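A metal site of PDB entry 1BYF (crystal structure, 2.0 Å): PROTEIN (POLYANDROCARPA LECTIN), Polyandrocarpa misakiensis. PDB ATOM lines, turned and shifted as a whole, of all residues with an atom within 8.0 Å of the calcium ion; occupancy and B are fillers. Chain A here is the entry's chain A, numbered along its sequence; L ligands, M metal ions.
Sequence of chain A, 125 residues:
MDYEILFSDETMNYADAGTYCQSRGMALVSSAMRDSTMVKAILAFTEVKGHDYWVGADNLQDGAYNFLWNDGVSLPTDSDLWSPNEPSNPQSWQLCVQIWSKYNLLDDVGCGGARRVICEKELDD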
ATOM      1  N   TYR A  65      23.532  -7.997  26.219  1.00  0.00           N
ATOM      2  CA  TYR A  65      24.135  -8.948  25.300  1.00  0.00           C
ATOM      3  C   TYR A  65      25.425  -9.512  25.906  1.00  0.00           C
ATOM      4  O   TYR A  65      26.406  -9.743  25.213  1.00  0.00           O
ATOM      5  CB  TYR A  65      24.343  -8.402  23.911  1.00  0.00           C
ATOM      6  CG  TYR A  65      23.103  -8.072  23.122  1.00  0.00           C
ATOM      7  CD1 TYR A  65      21.856  -8.604  23.437  1.00  0.00           C
ATOM      8  CD2 TYR A  65      23.181  -7.230  22.012  1.00  0.00           C
ATOM      9  CE1 TYR A  65      20.726  -8.306  22.701  1.00  0.00           C
ATOM     10  CE2 TYR A  65      22.053  -6.923  21.271  1.00  0.00           C
ATOM     11  CZ  TYR A  65      20.831  -7.458  21.613  1.00  0.00           C
ATOM     12  OH  TYR A  65      19.712  -7.147  20.882  1.00  0.00           O
ATOM     13  N   PHE A  67      26.081 -12.527  26.773  1.00  0.00           N
ATOM     14  CA  PHE A  67      25.690 -13.943  26.702  1.00  0.00           C
ATOM     15  C   PHE A  67      26.724 -14.863  27.320  1.00  0.00           C
ATOM     16  O   PHE A  67      27.911 -14.742  27.021  1.00  0.00           O
ATOM     17  CB  PHE A  67      25.423 -14.321  25.245  1.00  0.00           C
ATOM     18  CG  PHE A  67      24.098 -13.731  24.795  1.00  0.00           C
ATOM     19  CD1 PHE A  67      22.907 -14.347  25.130  1.00  0.00           C
ATOM     20  CD2 PHE A  67      24.063 -12.544  24.077  1.00  0.00           C
ATOM     21  CE1 PHE A  67      21.700 -13.798  24.739  1.00  0.00           C
ATOM     22  CE2 PHE A  67      22.866 -12.002  23.679  1.00  0.00           C
ATOM     23  CZ  PHE A  67      21.675 -12.618  24.014  1.00  0.00           C
ATOM     24  N   TRP A  82      26.178 -17.030  15.551  1.00  0.00           N
ATOM     25  CA  TRP A  82      24.925 -16.316  15.431  1.00  0.00           C
ATOM     26  C   TRP A  82      24.361 -16.272  14.011  1.00  0.00           C
ATOM     27  O   TRP A  82      25.090 -16.118  13.020  1.00  0.00           O
ATOM     28  CB  TRP A  82      25.064 -14.863  15.913  1.00  0.00           C
ATOM     29  CG  TRP A  82      25.406 -14.696  17.361  1.00  0.00           C
ATOM     30  CD1 TRP A  82      26.626 -14.393  17.891  1.00  0.00           C
ATOM     31  CD2 TRP A  82      24.506 -14.823  18.472  1.00  0.00           C
ATOM     32  NE1 TRP A  82      26.549 -14.326  19.255  1.00  0.00           N
ATOM     33  CE2 TRP A  82      25.256 -14.585  19.637  1.00  0.00           C
ATOM     34  CE3 TRP A  82      23.151 -15.117  18.601  1.00  0.00           C
ATOM     35  CZ2 TRP A  82      24.697 -14.628  20.916  1.00  0.00           C
ATOM     36  CZ3 TRP A  82      22.593 -15.169  19.863  1.00  0.00           C
ATOM     37  CH2 TRP A  82      23.361 -14.918  20.998  1.00  0.00           C
ATOM     38  N   SER A  83      23.036 -16.333  13.924  1.00  0.00           N
ATOM     39  CA  SER A  83      22.382 -16.183  12.631  1.00  0.00           C
ATOM     40  C   SER A  83      22.643 -14.737  12.184  1.00  0.00           C
ATOM     41  O   SER A  83      22.960 -13.900  13.023  1.00  0.00           O
ATOM     42  CB  SER A  83      20.875 -16.371  12.719  1.00  0.00           C
ATOM     43  OG  SER A  83      20.465 -17.559  13.349  1.00  0.00           O
ATOM     44  N   PRO A  84      22.473 -14.482  10.909  1.00  0.00           N
ATOM     45  CA  PRO A  84      22.611 -13.140  10.372  1.00  0.00           C
ATOM     46  C   PRO A  84      21.669 -12.198  11.113  1.00  0.00           C
ATOM     47  O   PRO A  84      20.491 -12.486  11.349  1.00  0.00           O
ATOM     48  CB  PRO A  84      22.226 -13.270   8.909  1.00  0.00           C
ATOM     49  CG  PRO A  84      22.366 -14.720   8.591  1.00  0.00           C
ATOM     50  CD  PRO A  84      22.068 -15.462   9.866  1.00  0.00           C
ATOM     51  N   ASN A  85      22.207 -11.057  11.526  1.00  0.00           N
ATOM     52  CA  ASN A  85      21.451 -10.022  12.218  1.00  0.00           C
ATOM     53  C   ASN A  85      20.940 -10.411  13.590  1.00  0.00           C
ATOM     54  O   ASN A  85      19.940  -9.853  14.064  1.00  0.00           O
ATOM     55  CB  ASN A  85      20.276  -9.533  11.364  1.00  0.00           C
ATOM     56  CG  ASN A  85      20.712  -8.996  10.014  1.00  0.00           C
ATOM     57  OD1 ASN A  85      20.107  -9.324   8.997  1.00  0.00           O
ATOM     58  ND2 ASN A  85      21.762  -8.175   9.998  1.00  0.00           N
ATOM     59  N   GLU A  86      21.613 -11.337  14.271  1.00  0.00           N
ATOM     60  CA  GLU A  86      21.257 -11.717  15.641  1.00  0.00           C
ATOM     61  C   GLU A  86      22.576 -11.657  16.405  1.00  0.00           C
ATOM     62  O   GLU A  86      23.616 -11.835  15.768  1.00  0.00           O
ATOM     63  CB  GLU A  86      20.628 -13.109  15.719  1.00  0.00           C
ATOM     64  CG  GLU A  86      19.369 -13.297  14.920  1.00  0.00           C
ATOM     65  CD  GLU A  86      18.176 -12.477  15.360  1.00  0.00           C
ATOM     66  OE1 GLU A  86      18.056 -12.118  16.559  1.00  0.00           O
ATOM     67  OE2 GLU A  86      17.309 -12.201  14.510  1.00  0.00           O
ATOM     68  N   PRO A  87      22.555 -11.421  17.697  1.00  0.00           N
ATOM     69  CA  PRO A  87      21.343 -11.211  18.462  1.00  0.00           C
ATOM     70  C   PRO A  87      20.697  -9.851  18.203  1.00  0.00           C
ATOM     71  O   PRO A  87      21.398  -8.884  17.905  1.00  0.00           O
ATOM     72  CB  PRO A  87      21.848 -11.272  19.910  1.00  0.00           C
ATOM     73  CG  PRO A  87      23.248 -10.751  19.825  1.00  0.00           C
ATOM     74  CD  PRO A  87      23.773 -11.329  18.537  1.00  0.00           C
ATOM     75  N   SER A  88      19.372  -9.769  18.345  1.00  0.00           N
ATOM     76  CA  SER A  88      18.708  -8.503  18.058  1.00  0.00           C
ATOM     77  C   SER A  88      17.509  -8.194  18.941  1.00  0.00           C
ATOM     78  O   SER A  88      16.843  -7.189  18.691  1.00  0.00           O
ATOM     79  CB  SER A  88      18.206  -8.580  16.599  1.00  0.00           C
ATOM     80  OG  SER A  88      17.171  -9.554  16.578  1.00  0.00           O
ATOM     81  N   ASN A  89      17.206  -9.041  19.927  1.00  0.00           N
ATOM     82  CA  ASN A  89      16.054  -8.785  20.799  1.00  0.00           C
ATOM     83  C   ASN A  89      16.412  -7.683  21.789  1.00  0.00           C
ATOM     84  O   ASN A  89      17.593  -7.395  22.008  1.00  0.00           O
ATOM     85  CB  ASN A  89      15.617 -10.065  21.505  1.00  0.00           C
ATOM     86  CG  ASN A  89      14.905 -11.042  20.583  1.00  0.00           C
ATOM     87  OD1 ASN A  89      15.346 -11.331  19.478  1.00  0.00           O
ATOM     88  ND2 ASN A  89      13.767 -11.565  21.043  1.00  0.00           N
ATOM     89  N   PRO A  90      15.418  -7.036  22.362  1.00  0.00           N
ATOM     90  CA  PRO A  90      15.653  -5.937  23.296  1.00  0.00           C
ATOM     91  C   PRO A  90      16.597  -6.346  24.419  1.00  0.00           C
ATOM     92  O   PRO A  90      16.383  -7.388  25.040  1.00  0.00           O
ATOM     93  CB  PRO A  90      14.265  -5.570  23.788  1.00  0.00           C
ATOM     94  CG  PRO A  90      13.334  -6.073  22.740  1.00  0.00           C
ATOM     95  CD  PRO A  90      13.982  -7.304  22.154  1.00  0.00           C
ATOM     96  N   TRP A  93      15.380  -7.529  28.061  1.00  0.00           N
ATOM     97  CA  TRP A  93      14.766  -8.829  28.307  1.00  0.00           C
ATOM     98  C   TRP A  93      15.745  -9.875  28.844  1.00  0.00           C
ATOM     99  O   TRP A  93      16.952  -9.813  28.616  1.00  0.00           O
ATOM    100  CB  TRP A  93      14.232  -9.440  27.011  1.00  0.00           C
ATOM    101  CG  TRP A  93      13.123  -8.745  26.297  1.00  0.00           C
ATOM    102  CD1 TRP A  93      12.649  -7.483  26.496  1.00  0.00           C
ATOM    103  CD2 TRP A  93      12.368  -9.295  25.200  1.00  0.00           C
ATOM    104  NE1 TRP A  93      11.631  -7.222  25.617  1.00  0.00           N
ATOM    105  CE2 TRP A  93      11.436  -8.321  24.804  1.00  0.00           C
ATOM    106  CE3 TRP A  93      12.385 -10.526  24.532  1.00  0.00           C
ATOM    107  CZ2 TRP A  93      10.533  -8.529  23.770  1.00  0.00           C
ATOM    108  CZ3 TRP A  93      11.492 -10.736  23.500  1.00  0.00           C
ATOM    109  CH2 TRP A  93      10.570  -9.739  23.126  1.00  0.00           C
ATOM    110  N   LEU A  95      17.210 -13.050  28.016  1.00  0.00           N
ATOM    111  CA  LEU A  95      17.330 -13.726  26.737  1.00  0.00           C
ATOM    112  C   LEU A  95      18.054 -15.062  26.803  1.00  0.00           C
ATOM    113  O   LEU A  95      19.100 -15.207  27.442  1.00  0.00           O
ATOM    114  CB  LEU A  95      18.027 -12.799  25.728  1.00  0.00           C
ATOM    115  CG  LEU A  95      17.278 -11.476  25.505  1.00  0.00           C
ATOM    116  CD1 LEU A  95      18.215 -10.447  24.900  1.00  0.00           C
ATOM    117  CD2 LEU A  95      16.049 -11.696  24.622  1.00  0.00           C
ATOM    118  N   CYS A  96      17.446 -16.025  26.116  1.00  0.00           N
ATOM    119  CA  CYS A  96      17.968 -17.388  26.028  1.00  0.00           C
ATOM    120  C   CYS A  96      18.367 -17.669  24.588  1.00  0.00           C
ATOM    121  O   CYS A  96      17.897 -16.966  23.684  1.00  0.00           O
ATOM    122  CB  CYS A  96      16.884 -18.365  26.517  1.00  0.00           C
ATOM    123  SG  CYS A  96      16.675 -18.203  28.302  1.00  0.00           S
ATOM    124  N   GLN A  98      18.890 -20.217  21.225  1.00  0.00           N
ATOM    125  CA  GLN A  98      18.457 -21.401  20.533  1.00  0.00           C
ATOM    126  C   GLN A  98      19.187 -21.528  19.196  1.00  0.00           C
ATOM    127  O   GLN A  98      19.815 -20.596  18.702  1.00  0.00           O
ATOM    128  CB  GLN A  98      16.955 -21.323  20.161  1.00  0.00           C
ATOM    129  CG  GLN A  98      16.689 -20.121  19.249  1.00  0.00           C
ATOM    130  CD  GLN A  98      15.421 -20.246  18.434  1.00  0.00           C
ATOM    131  OE1 GLN A  98      14.766 -21.280  18.426  1.00  0.00           O
ATOM    132  NE2 GLN A  98      15.072 -19.189  17.706  1.00  0.00           N
ATOM    133  N   TRP A 100      18.097 -21.597  15.788  1.00  0.00           N
ATOM    134  CA  TRP A 100      16.911 -21.177  15.056  1.00  0.00           C
ATOM    135  C   TRP A 100      16.777 -21.855  13.707  1.00  0.00           C
ATOM    136  O   TRP A 100      17.685 -21.755  12.882  1.00  0.00           O
ATOM    137  CB  TRP A 100      16.998 -19.654  14.897  1.00  0.00           C
ATOM    138  CG  TRP A 100      15.831 -18.965  14.274  1.00  0.00           C
ATOM    139  CD1 TRP A 100      14.563 -19.426  14.126  1.00  0.00           C
ATOM    140  CD2 TRP A 100      15.833 -17.629  13.751  1.00  0.00           C
ATOM    141  NE1 TRP A 100      13.777 -18.475  13.524  1.00  0.00           N
ATOM    142  CE2 TRP A 100      14.538 -17.360  13.285  1.00  0.00           C
ATOM    143  CE3 TRP A 100      16.823 -16.646  13.623  1.00  0.00           C
ATOM    144  CZ2 TRP A 100      14.187 -16.143  12.694  1.00  0.00           C
ATOM    145  CZ3 TRP A 100      16.470 -15.437  13.037  1.00  0.00           C
ATOM    146  CH2 TRP A 100      15.160 -15.193  12.583  1.00  0.00           C
ATOM    147  N   LEU A 106      22.579 -19.764  15.715  1.00  0.00           N
ATOM    148  CA  LEU A 106      22.117 -19.250  17.000  1.00  0.00           C
ATOM    149  C   LEU A 106      21.264 -17.996  16.901  1.00  0.00           C
ATOM    150  O   LEU A 106      21.375 -17.181  15.985  1.00  0.00           O
ATOM    151  CB  LEU A 106      23.302 -19.043  17.945  1.00  0.00           C
ATOM    152  CG  LEU A 106      24.190 -20.247  18.228  1.00  0.00           C
ATOM    153  CD1 LEU A 106      25.174 -19.876  19.336  1.00  0.00           C
ATOM    154  CD2 LEU A 106      23.391 -21.475  18.647  1.00  0.00           C
ATOM    155  N   ASP A 107      20.391 -17.852  17.900  1.00  0.00           N
ATOM    156  CA  ASP A 107      19.486 -16.715  17.946  1.00  0.00           C
ATOM    157  C   ASP A 107      19.032 -16.470  19.380  1.00  0.00           C
ATOM    158  O   ASP A 107      18.876 -17.437  20.136  1.00  0.00           O
ATOM    159  CB  ASP A 107      18.300 -16.984  17.016  1.00  0.00           C
ATOM    160  CG  ASP A 107      17.163 -15.999  17.212  1.00  0.00           C
ATOM    161  OD1 ASP A 107      17.460 -14.777  17.192  1.00  0.00           O
ATOM    162  OD2 ASP A 107      16.013 -16.438  17.400  1.00  0.00           O
ATOM    163  N   ASP A 108      18.818 -15.208  19.731  1.00  0.00           N
ATOM    164  CA  ASP A 108      18.337 -14.856  21.053  1.00  0.00           C
ATOM    165  C   ASP A 108      16.805 -14.770  21.033  1.00  0.00           C
ATOM    166  O   ASP A 108      16.212 -14.216  20.125  1.00  0.00           O
ATOM    167  CB  ASP A 108      18.913 -13.540  21.563  1.00  0.00           C
ATOM    168  CG  ASP A 108      18.654 -12.338  20.674  1.00  0.00           C
ATOM    169  OD1 ASP A 108      18.515 -12.465  19.443  1.00  0.00           O
ATOM    170  OD2 ASP A 108      18.607 -11.229  21.238  1.00  0.00           O
ATOM    171  N   VAL A 109      16.185 -15.360  22.048  1.00  0.00           N
ATOM    172  CA  VAL A 109      14.746 -15.374  22.179  1.00  0.00           C
ATOM    173  C   VAL A 109      14.366 -15.207  23.653  1.00  0.00           C
ATOM    174  O   VAL A 109      15.236 -15.302  24.514  1.00  0.00           O
ATOM    175  CB  VAL A 109      14.148 -16.722  21.708  1.00  0.00           C
ATOM    176  CG1 VAL A 109      14.259 -16.878  20.202  1.00  0.00           C
ATOM    177  CG2 VAL A 109      14.858 -17.888  22.396  1.00  0.00           C
ATOM    178  N   GLY A 110      13.074 -15.028  23.917  1.00  0.00           N
ATOM    179  CA  GLY A 110      12.600 -14.983  25.303  1.00  0.00           C
ATOM    180  C   GLY A 110      12.769 -16.421  25.821  1.00  0.00           C
ATOM    181  O   GLY A 110      13.005 -17.313  24.995  1.00  0.00           O
HETATM  182  C1  LIG L   1      13.571 -12.054  14.843  1.00  0.00           C
HETATM  183  O1  LIG L   1      13.027 -10.782  14.925  1.00  0.00           O
HETATM  184  C2  LIG L   1      14.161 -12.435  16.197  1.00  0.00           C
HETATM  185  O2  LIG L   1      15.438 -11.834  16.345  1.00  0.00           O
HETATM  186  C3  LIG L   1      14.297 -13.951  16.256  1.00  0.00           C
HETATM  187  O3  LIG L   1      14.657 -14.287  17.550  1.00  0.00           O
HETATM  188 CA    CA M   1      16.660 -12.875  18.066  1.00  0.00          CA
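O of Asn 89 lies within hydrogen-bond range of OH of Tyr 65 (2.4 Å). The backbone carbonyl oxygen (O) of Gln 98 is in hydrogen-bond range of the backbone NH (N) of Asp 107, at 2.9 Å. The backbone NH (N) of Ser 88 lies within hydrogen-bond range of the side-chain carboxylate (OD2) of Asp 108, 3.3 Å away. OE2 of Glu 86 sits close to OG of Ser 88 (3.4 Å).
Residues that only touch the calcium ion: Ser 88 (3.7 Å).
The calcium ion is bound by the side-chain carboxylate of Glu 86 (2.2 Å), the side-chain carboxylate of Asp 107 (2.2 Å), the side-chain carboxylate of Asp 108 (2.3 Å), an oxygen (O2) of the ligand (2.4 Å), the side-chain amide oxygen of Asn 89 (2.5 Å), the backbone carbonyl oxygen of Asp 108 (2.5 Å) and an oxygen (O3) of the ligand (2.5 Å).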
